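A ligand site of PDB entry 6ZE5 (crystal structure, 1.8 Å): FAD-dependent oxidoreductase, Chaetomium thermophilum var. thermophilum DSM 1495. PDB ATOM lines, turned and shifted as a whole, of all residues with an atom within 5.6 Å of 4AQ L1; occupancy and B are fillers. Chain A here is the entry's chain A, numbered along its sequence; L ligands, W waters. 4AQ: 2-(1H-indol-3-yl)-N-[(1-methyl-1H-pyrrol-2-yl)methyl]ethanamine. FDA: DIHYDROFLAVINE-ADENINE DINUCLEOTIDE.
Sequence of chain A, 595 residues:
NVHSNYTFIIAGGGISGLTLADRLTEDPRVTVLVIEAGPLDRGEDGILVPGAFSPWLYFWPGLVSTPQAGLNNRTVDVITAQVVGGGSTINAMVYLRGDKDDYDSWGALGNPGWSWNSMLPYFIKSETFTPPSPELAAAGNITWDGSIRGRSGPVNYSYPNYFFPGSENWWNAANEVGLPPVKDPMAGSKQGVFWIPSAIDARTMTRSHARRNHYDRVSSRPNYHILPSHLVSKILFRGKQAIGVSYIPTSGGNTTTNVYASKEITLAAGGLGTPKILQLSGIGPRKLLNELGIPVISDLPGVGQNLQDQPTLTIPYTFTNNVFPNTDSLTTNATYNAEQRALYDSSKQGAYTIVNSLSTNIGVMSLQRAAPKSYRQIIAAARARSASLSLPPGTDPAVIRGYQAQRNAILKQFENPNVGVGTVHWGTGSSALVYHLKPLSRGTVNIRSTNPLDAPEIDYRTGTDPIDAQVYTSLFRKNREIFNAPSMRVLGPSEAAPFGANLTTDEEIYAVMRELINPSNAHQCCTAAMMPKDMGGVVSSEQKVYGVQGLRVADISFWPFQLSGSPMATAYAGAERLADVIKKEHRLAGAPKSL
OH of Tyr 435 sits at hydrogen-bond distance from N1 of 4AQ L1, at 2.8 Å.
OD1 of Asn 521 is in hydrogen-bond range of N1 of 4AQ L1 (3.0 Å).
The backbone NH (N) of Ala 92 sits close to an oxygen (O4) of FDA L2 (3.3 Å).
An oxygen (O4) of FDA L2 is in hydrogen-bond range of the backbone NH (N) of Val 94 (3.1 Å).
A nitrogen (N3) of FDA L2 is in hydrogen-bond range of the backbone carbonyl oxygen (O) of Val 94 (2.8 Å).
An oxygen (O2) of FDA L2 sits close to the side-chain hydroxyl (OG) of Ser 566 (3.2 Å).
Water W3 lies within hydrogen-bond range of a ring nitrogen (NE2) of His 523 (2.7 Å), the side-chain amide oxygen of Asn 521 (2.8 Å), a nitrogen (N1) of 4AQ L1 (2.9 Å) and a nitrogen (N5) of FDA L2 (3.1 Å).
The backbone NH (N) of Tyr 435 is in hydrogen-bond range of the backbone carbonyl oxygen (O) of Thr 423 (2.8 Å).
Phe 53 touches 4AQ L1.
CG of Pro 55 touches N2 of 4AQ L1 (3.8 Å).
CZ of Phe 59 touches C15 of 4AQ L1, 3.96 Å away.
Ile 79 touches 4AQ L1.
Ala 92 touches 4AQ L1 (CB to C5, 3.5 Å).
Val 94 touches 4AQ L1.
Ile 362 touches 4AQ L1.
His 523 touches 4AQ L1 (CE1 to C, 3.9 Å).
Ser 566 touches 4AQ L1 (CB to C, 3.8 Å).
Within 4 Å of 4AQ L1: Phe 53, Pro 55, Phe 59, Ile 79, Ala 92, Val 94, Ile 362, Tyr 435, Asn 521, His 523 and Ser 566.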
ATOM      1  N   PHE A  53      -0.722 -21.459  17.701  1.00  0.00           N
ATOM      2  CA  PHE A  53      -0.054 -21.924  16.476  1.00  0.00           C
ATOM      3  C   PHE A  53       0.581 -23.321  16.541  1.00  0.00           C
ATOM      4  O   PHE A  53       1.519 -23.540  17.316  1.00  0.00           O
ATOM      5  CB  PHE A  53       0.996 -20.875  16.092  1.00  0.00           C
ATOM      6  CG  PHE A  53       1.734 -21.151  14.814  1.00  0.00           C
ATOM      7  CD1 PHE A  53       1.049 -21.506  13.665  1.00  0.00           C
ATOM      8  CD2 PHE A  53       3.120 -20.993  14.760  1.00  0.00           C
ATOM      9  CE1 PHE A  53       1.766 -21.718  12.471  1.00  0.00           C
ATOM     10  CE2 PHE A  53       3.838 -21.206  13.566  1.00  0.00           C
ATOM     11  CZ  PHE A  53       3.156 -21.566  12.425  1.00  0.00           C
ATOM     12  N   PRO A  55       1.724 -25.613  13.559  1.00  0.00           N
ATOM     13  CA  PRO A  55       1.835 -25.895  12.119  1.00  0.00           C
ATOM     14  C   PRO A  55       1.999 -27.378  11.810  1.00  0.00           C
ATOM     15  O   PRO A  55       1.489 -27.832  10.777  1.00  0.00           O
ATOM     16  CB  PRO A  55       3.067 -25.087  11.701  1.00  0.00           C
ATOM     17  CG  PRO A  55       3.903 -24.960  13.010  1.00  0.00           C
ATOM     18  CD  PRO A  55       2.807 -24.758  14.047  1.00  0.00           C
ATOM     19  N   PHE A  59       1.798 -30.945   8.299  1.00  0.00           N
ATOM     20  CA  PHE A  59       3.035 -31.196   7.569  1.00  0.00           C
ATOM     21  C   PHE A  59       2.884 -32.412   6.636  1.00  0.00           C
ATOM     22  O   PHE A  59       2.289 -33.429   6.997  1.00  0.00           O
ATOM     23  CB  PHE A  59       4.170 -31.433   8.560  1.00  0.00           C
ATOM     24  CG  PHE A  59       4.645 -30.187   9.314  1.00  0.00           C
ATOM     25  CD1 PHE A  59       4.211 -28.916   8.953  1.00  0.00           C
ATOM     26  CD2 PHE A  59       5.547 -30.308  10.373  1.00  0.00           C
ATOM     27  CE1 PHE A  59       4.679 -27.796   9.659  1.00  0.00           C
ATOM     28  CE2 PHE A  59       6.027 -29.201  11.065  1.00  0.00           C
ATOM     29  CZ  PHE A  59       5.585 -27.942  10.702  1.00  0.00           C
ATOM     30  N   ILE A  79       9.714 -29.703   5.176  1.00  0.00           N
ATOM     31  CA  ILE A  79       8.449 -29.167   5.704  1.00  0.00           C
ATOM     32  C   ILE A  79       7.718 -28.471   4.556  1.00  0.00           C
ATOM     33  O   ILE A  79       8.221 -27.509   3.966  1.00  0.00           O
ATOM     34  CB  ILE A  79       8.679 -28.195   6.879  1.00  0.00           C
ATOM     35  CG1 ILE A  79       9.534 -28.843   7.978  1.00  0.00           C
ATOM     36  CG2 ILE A  79       7.353 -27.701   7.457  1.00  0.00           C
ATOM     37  CD1 ILE A  79       9.072 -30.223   8.352  1.00  0.00           C
ATOM     38  N   ALA A  92       3.290 -19.013   9.435  1.00  0.00           N
ATOM     39  CA  ALA A  92       3.403 -18.046  10.520  1.00  0.00           C
ATOM     40  C   ALA A  92       2.631 -16.744  10.221  1.00  0.00           C
ATOM     41  O   ALA A  92       2.750 -15.754  10.959  1.00  0.00           O
ATOM     42  CB  ALA A  92       4.896 -17.743  10.781  1.00  0.00           C
ATOM     43  N   VAL A  94       3.080 -14.377   8.264  1.00  0.00           N
ATOM     44  CA  VAL A  94       3.868 -13.218   7.857  1.00  0.00           C
ATOM     45  C   VAL A  94       3.532 -12.863   6.415  1.00  0.00           C
ATOM     46  O   VAL A  94       3.710 -13.674   5.486  1.00  0.00           O
ATOM     47  CB  VAL A  94       5.365 -13.503   8.025  1.00  0.00           C
ATOM     48  CG1 VAL A  94       6.227 -12.336   7.492  1.00  0.00           C
ATOM     49  CG2 VAL A  94       5.679 -13.838   9.487  1.00  0.00           C
ATOM     50  N   ILE A 196       5.509  -6.426  11.511  1.00  0.00           N
ATOM     51  CA  ILE A 196       5.156  -7.526  10.596  1.00  0.00           C
ATOM     52  C   ILE A 196       3.676  -7.458  10.230  1.00  0.00           C
ATOM     53  O   ILE A 196       2.835  -7.587  11.111  1.00  0.00           O
ATOM     54  CB  ILE A 196       5.433  -8.878  11.270  1.00  0.00           C
ATOM     55  CG1 ILE A 196       6.891  -9.063  11.625  1.00  0.00           C
ATOM     56  CG2 ILE A 196       4.926 -10.027  10.415  1.00  0.00           C
ATOM     57  CD1 ILE A 196       7.083 -10.228  12.620  1.00  0.00           C
ATOM     58  N   LEU A 358       6.635 -15.743  17.972  1.00  0.00           N
ATOM     59  CA  LEU A 358       7.046 -14.541  17.254  1.00  0.00           C
ATOM     60  C   LEU A 358       6.837 -13.290  18.111  1.00  0.00           C
ATOM     61  O   LEU A 358       6.118 -13.300  19.112  1.00  0.00           O
ATOM     62  CB  LEU A 358       6.281 -14.361  15.950  1.00  0.00           C
ATOM     63  CG  LEU A 358       6.383 -15.426  14.877  1.00  0.00           C
ATOM     64  CD1 LEU A 358       5.710 -14.868  13.623  1.00  0.00           C
ATOM     65  CD2 LEU A 358       7.868 -15.779  14.651  1.00  0.00           C
ATOM     66  N   ILE A 362      10.256  -6.572  12.935  1.00  0.00           N
ATOM     67  CA  ILE A 362      11.227  -7.356  12.172  1.00  0.00           C
ATOM     68  C   ILE A 362      12.096  -6.383  11.386  1.00  0.00           C
ATOM     69  O   ILE A 362      11.735  -5.222  11.190  1.00  0.00           O
ATOM     70  CB  ILE A 362      10.469  -8.333  11.241  1.00  0.00           C
ATOM     71  CG1 ILE A 362      11.389  -9.455  10.781  1.00  0.00           C
ATOM     72  CG2 ILE A 362       9.866  -7.552  10.065  1.00  0.00           C
ATOM     73  CD1 ILE A 362      10.597 -10.637  10.211  1.00  0.00           C
ATOM     74  N   THR A 423      16.968 -11.135   6.748  1.00  0.00           N
ATOM     75  CA  THR A 423      15.953 -10.779   7.733  1.00  0.00           C
ATOM     76  C   THR A 423      16.469 -11.097   9.121  1.00  0.00           C
ATOM     77  O   THR A 423      17.124 -12.124   9.323  1.00  0.00           O
ATOM     78  CB  THR A 423      14.648 -11.565   7.477  1.00  0.00           C
ATOM     79  OG1 THR A 423      14.130 -11.236   6.183  1.00  0.00           O
ATOM     80  CG2 THR A 423      13.611 -11.198   8.514  1.00  0.00           C
ATOM     81  N   HIS A 425      15.109 -11.129  13.383  1.00  0.00           N
ATOM     82  CA  HIS A 425      13.908 -11.134  14.217  1.00  0.00           C
ATOM     83  C   HIS A 425      14.288 -11.606  15.608  1.00  0.00           C
ATOM     84  O   HIS A 425      15.146 -12.468  15.786  1.00  0.00           O
ATOM     85  CB  HIS A 425      12.828 -12.028  13.606  1.00  0.00           C
ATOM     86  CG  HIS A 425      11.546 -12.057  14.385  1.00  0.00           C
ATOM     87  ND1 HIS A 425      10.699 -10.987  14.462  1.00  0.00           N
ATOM     88  CD2 HIS A 425      10.955 -13.046  15.108  1.00  0.00           C
ATOM     89  CE1 HIS A 425       9.655 -11.297  15.210  1.00  0.00           C
ATOM     90  NE2 HIS A 425       9.791 -12.540  15.612  1.00  0.00           N
ATOM     91  N   LEU A 433      16.270 -15.080  15.219  1.00  0.00           N
ATOM     92  CA  LEU A 433      16.137 -15.696  13.907  1.00  0.00           C
ATOM     93  C   LEU A 433      16.841 -14.836  12.873  1.00  0.00           C
ATOM     94  O   LEU A 433      16.589 -13.621  12.800  1.00  0.00           O
ATOM     95  CB  LEU A 433      14.665 -15.859  13.510  1.00  0.00           C
ATOM     96  CG  LEU A 433      13.713 -16.630  14.428  1.00  0.00           C
ATOM     97  CD1 LEU A 433      12.250 -16.553  13.961  1.00  0.00           C
ATOM     98  CD2 LEU A 433      14.126 -18.061  14.590  1.00  0.00           C
ATOM     99  N   TYR A 435      17.386 -14.882   8.684  1.00  0.00           N
ATOM    100  CA  TYR A 435      16.906 -15.515   7.469  1.00  0.00           C
ATOM    101  C   TYR A 435      17.759 -15.042   6.305  1.00  0.00           C
ATOM    102  O   TYR A 435      17.945 -13.831   6.131  1.00  0.00           O
ATOM    103  CB  TYR A 435      15.452 -15.168   7.197  1.00  0.00           C
ATOM    104  CG  TYR A 435      14.476 -15.823   8.156  1.00  0.00           C
ATOM    105  CD1 TYR A 435      14.873 -16.864   9.003  1.00  0.00           C
ATOM    106  CD2 TYR A 435      13.173 -15.395   8.215  1.00  0.00           C
ATOM    107  CE1 TYR A 435      13.960 -17.448   9.866  1.00  0.00           C
ATOM    108  CE2 TYR A 435      12.266 -15.972   9.068  1.00  0.00           C
ATOM    109  CZ  TYR A 435      12.659 -16.990   9.880  1.00  0.00           C
ATOM    110  OH  TYR A 435      11.693 -17.541  10.699  1.00  0.00           O
ATOM    111  N   SER A 520      15.741 -24.577   4.886  1.00  0.00           N
ATOM    112  CA  SER A 520      14.402 -24.296   4.390  1.00  0.00           C
ATOM    113  C   SER A 520      13.558 -23.591   5.449  1.00  0.00           C
ATOM    114  O   SER A 520      13.545 -23.999   6.621  1.00  0.00           O
ATOM    115  CB  SER A 520      13.739 -25.608   3.973  1.00  0.00           C
ATOM    116  OG  SER A 520      12.356 -25.416   3.715  1.00  0.00           O
ATOM    117  N   ASN A 521      12.870 -22.529   5.021  1.00  0.00           N
ATOM    118  CA  ASN A 521      11.811 -21.901   5.802  1.00  0.00           C
ATOM    119  C   ASN A 521      10.425 -22.441   5.429  1.00  0.00           C
ATOM    120  O   ASN A 521       9.414 -21.832   5.808  1.00  0.00           O
ATOM    121  CB  ASN A 521      11.842 -20.377   5.595  1.00  0.00           C
ATOM    122  CG  ASN A 521      11.551 -19.578   6.886  1.00  0.00           C
ATOM    123  OD1 ASN A 521      11.125 -20.132   7.897  1.00  0.00           O
ATOM    124  ND2 ASN A 521      11.814 -18.279   6.832  1.00  0.00           N
ATOM    125  N   ALA A 522      10.355 -23.541   4.668  1.00  0.00           N
ATOM    126  CA  ALA A 522       9.167 -24.004   3.962  1.00  0.00           C
ATOM    127  C   ALA A 522       8.748 -23.022   2.867  1.00  0.00           C
ATOM    128  O   ALA A 522       7.566 -22.900   2.557  1.00  0.00           O
ATOM    129  CB  ALA A 522       8.012 -24.291   4.906  1.00  0.00           C
ATOM    130  N   HIS A 523       9.722 -22.345   2.281  1.00  0.00           N
ATOM    131  CA  HIS A 523       9.519 -21.422   1.159  1.00  0.00           C
ATOM    132  C   HIS A 523       9.940 -22.009  -0.171  1.00  0.00           C
ATOM    133  O   HIS A 523      10.467 -21.256  -1.007  1.00  0.00           O
ATOM    134  CB  HIS A 523      10.303 -20.128   1.391  1.00  0.00           C
ATOM    135  CG  HIS A 523       9.831 -19.354   2.569  1.00  0.00           C
ATOM    136  ND1 HIS A 523      10.367 -18.137   2.921  1.00  0.00           N
ATOM    137  CD2 HIS A 523       8.851 -19.611   3.470  1.00  0.00           C
ATOM    138  CE1 HIS A 523       9.752 -17.685   3.992  1.00  0.00           C
ATOM    139  NE2 HIS A 523       8.822 -18.553   4.347  1.00  0.00           N
ATOM    140  N   SER A 566       9.197 -13.037   2.379  1.00  0.00           N
ATOM    141  CA  SER A 566       8.541 -14.334   2.363  1.00  0.00           C
ATOM    142  C   SER A 566       7.507 -14.402   1.235  1.00  0.00           C
ATOM    143  O   SER A 566       7.016 -13.377   0.777  1.00  0.00           O
ATOM    144  CB  SER A 566       7.882 -14.588   3.713  1.00  0.00           C
ATOM    145  OG  SER A 566       7.243 -13.434   4.222  1.00  0.00           O
HETATM  146  C4  4AQ L   1       8.735 -16.183   9.754  1.00  0.00           C
HETATM  147  C5  4AQ L   1       8.213 -17.588   9.804  1.00  0.00           C
HETATM  148  C6  4AQ L   1       9.098 -19.747  10.535  1.00  0.00           C
HETATM  149  N1  4AQ L   1       9.301 -18.558   9.698  1.00  0.00           N
HETATM  150  C7  4AQ L   1       7.782 -20.453  10.245  1.00  0.00           C
HETATM  151  C8  4AQ L   1       7.762 -21.841  10.800  1.00  0.00           C
HETATM  152  N2  4AQ L   1       7.358 -23.631  12.106  1.00  0.00           N
HETATM  153  C9  4AQ L   1       7.152 -22.279  11.945  1.00  0.00           C
HETATM  154  C10 4AQ L   1       8.121 -24.097  11.051  1.00  0.00           C
HETATM  155  C11 4AQ L   1       8.401 -22.989  10.208  1.00  0.00           C
HETATM  156  C12 4AQ L   1       9.183 -23.200   9.061  1.00  0.00           C
HETATM  157  C13 4AQ L   1       9.658 -24.466   8.801  1.00  0.00           C
HETATM  158  C14 4AQ L   1       9.372 -25.545   9.652  1.00  0.00           C
HETATM  159  C15 4AQ L   1       8.602 -25.385  10.787  1.00  0.00           C
HETATM  160  C   4AQ L   1       8.518 -15.979   7.245  1.00  0.00           C
HETATM  161  N   4AQ L   1       8.857 -15.502   8.574  1.00  0.00           N
HETATM  162  C3  4AQ L   1       9.153 -15.360  10.774  1.00  0.00           C
HETATM  163  C2  4AQ L   1       9.536 -14.141  10.226  1.00  0.00           C
HETATM  164  C1  4AQ L   1       9.363 -14.222   8.877  1.00  0.00           C
HETATM  165  PA  FDA L   2       1.043 -24.407  -1.210  1.00  0.00           P
HETATM  166  O1A FDA L   2       2.055 -25.235  -0.482  1.00  0.00           O
HETATM  167  O2A FDA L   2       0.294 -23.362  -0.448  1.00  0.00           O
HETATM  168  O5B FDA L   2      -0.042 -25.348  -1.898  1.00  0.00           O
HETATM  169  C5B FDA L   2       0.334 -26.580  -2.529  1.00  0.00           C
HETATM  170  C4B FDA L   2      -0.747 -27.585  -2.217  1.00  0.00           C
HETATM  171  O4B FDA L   2      -0.642 -28.670  -3.167  1.00  0.00           O
HETATM  172  C3B FDA L   2      -0.702 -28.226  -0.824  1.00  0.00           C
HETATM  173  O3B FDA L   2      -1.926 -27.988  -0.144  1.00  0.00           O
HETATM  174  C2B FDA L   2      -0.473 -29.728  -1.109  1.00  0.00           C
HETATM  175  O2B FDA L   2      -1.186 -30.586  -0.245  1.00  0.00           O
HETATM  176  C1B FDA L   2      -1.022 -29.862  -2.530  1.00  0.00           C
HETATM  177  N9A FDA L   2      -0.459 -30.926  -3.375  1.00  0.00           N
HETATM  178  C8A FDA L   2       0.856 -31.220  -3.619  1.00  0.00           C
HETATM  179  N7A FDA L   2       1.021 -32.192  -4.489  1.00  0.00           N
HETATM  180  C5A FDA L   2      -0.279 -32.522  -4.870  1.00  0.00           C
HETATM  181  C6A FDA L   2      -0.793 -33.478  -5.781  1.00  0.00           C
HETATM  182  N6A FDA L   2      -0.038 -34.301  -6.513  1.00  0.00           N
HETATM  183  N1A FDA L   2      -2.146 -33.550  -5.888  1.00  0.00           N
HETATM  184  C2A FDA L   2      -2.902 -32.718  -5.150  1.00  0.00           C
HETATM  185  N3A FDA L   2      -2.537 -31.789  -4.267  1.00  0.00           N
HETATM  186  C4A FDA L   2      -1.193 -31.740  -4.183  1.00  0.00           C
HETATM  187  N1  FDA L   2       5.211 -17.717   3.822  1.00  0.00           N
HETATM  188  C2  FDA L   2       5.059 -16.398   4.201  1.00  0.00           C
HETATM  189  O2  FDA L   2       4.967 -15.519   3.353  1.00  0.00           O
HETATM  190  N3  FDA L   2       4.995 -16.134   5.549  1.00  0.00           N
HETATM  191  C4  FDA L   2       5.097 -17.100   6.551  1.00  0.00           C
HETATM  192  O4  FDA L   2       5.046 -16.756   7.742  1.00  0.00           O
HETATM  193  C4X FDA L   2       5.311 -18.444   6.131  1.00  0.00           C
HETATM  194  N5  FDA L   2       5.518 -19.457   7.025  1.00  0.00           N
HETATM  195  C5X FDA L   2       5.450 -20.781   6.661  1.00  0.00           C
HETATM  196  C6  FDA L   2       5.388 -21.775   7.616  1.00  0.00           C
HETATM  197  C7  FDA L   2       5.194 -23.085   7.276  1.00  0.00           C
HETATM  198  C7M FDA L   2       5.133 -24.132   8.348  1.00  0.00           C
HETATM  199  C8  FDA L   2       5.026 -23.429   5.892  1.00  0.00           C
HETATM  200  C8M FDA L   2       4.794 -24.868   5.503  1.00  0.00           C
HETATM  201  C9  FDA L   2       5.089 -22.443   4.931  1.00  0.00           C
HETATM  202  C9A FDA L   2       5.305 -21.104   5.304  1.00  0.00           C
HETATM  203  N10 FDA L   2       5.406 -20.066   4.346  1.00  0.00           N
HETATM  204  C10 FDA L   2       5.319 -18.737   4.741  1.00  0.00           C
HETATM  205  C1' FDA L   2       5.501 -20.399   2.908  1.00  0.00           C
HETATM  206  C2' FDA L   2       4.229 -20.126   2.144  1.00  0.00           C
HETATM  207  O2' FDA L   2       3.077 -20.504   2.897  1.00  0.00           O
HETATM  208  C3' FDA L   2       4.313 -20.969   0.876  1.00  0.00           C
HETATM  209  O3' FDA L   2       5.448 -20.597   0.091  1.00  0.00           O
HETATM  210  C4' FDA L   2       3.074 -20.897   0.004  1.00  0.00           C
HETATM  211  O4' FDA L   2       1.956 -21.395   0.745  1.00  0.00           O
HETATM  212  C5' FDA L   2       3.274 -21.721  -1.251  1.00  0.00           C
HETATM  213  O5' FDA L   2       2.123 -21.403  -2.076  1.00  0.00           O
HETATM  214  P   FDA L   2       1.720 -22.385  -3.272  1.00  0.00           P
HETATM  215  O1P FDA L   2       0.344 -22.066  -3.742  1.00  0.00           O
HETATM  216  O2P FDA L   2       2.888 -22.332  -4.224  1.00  0.00           O
HETATM  217  O3P FDA L   2       1.759 -23.783  -2.488  1.00  0.00           O
HETATM  218  O   HOH W   1       9.590 -22.943  14.660  1.00  0.00           O
HETATM  219  O   HOH W   2      11.848 -21.685   9.948  1.00  0.00           O
HETATM  220  O   HOH W   3       8.608 -19.227   6.931  1.00  0.00           O
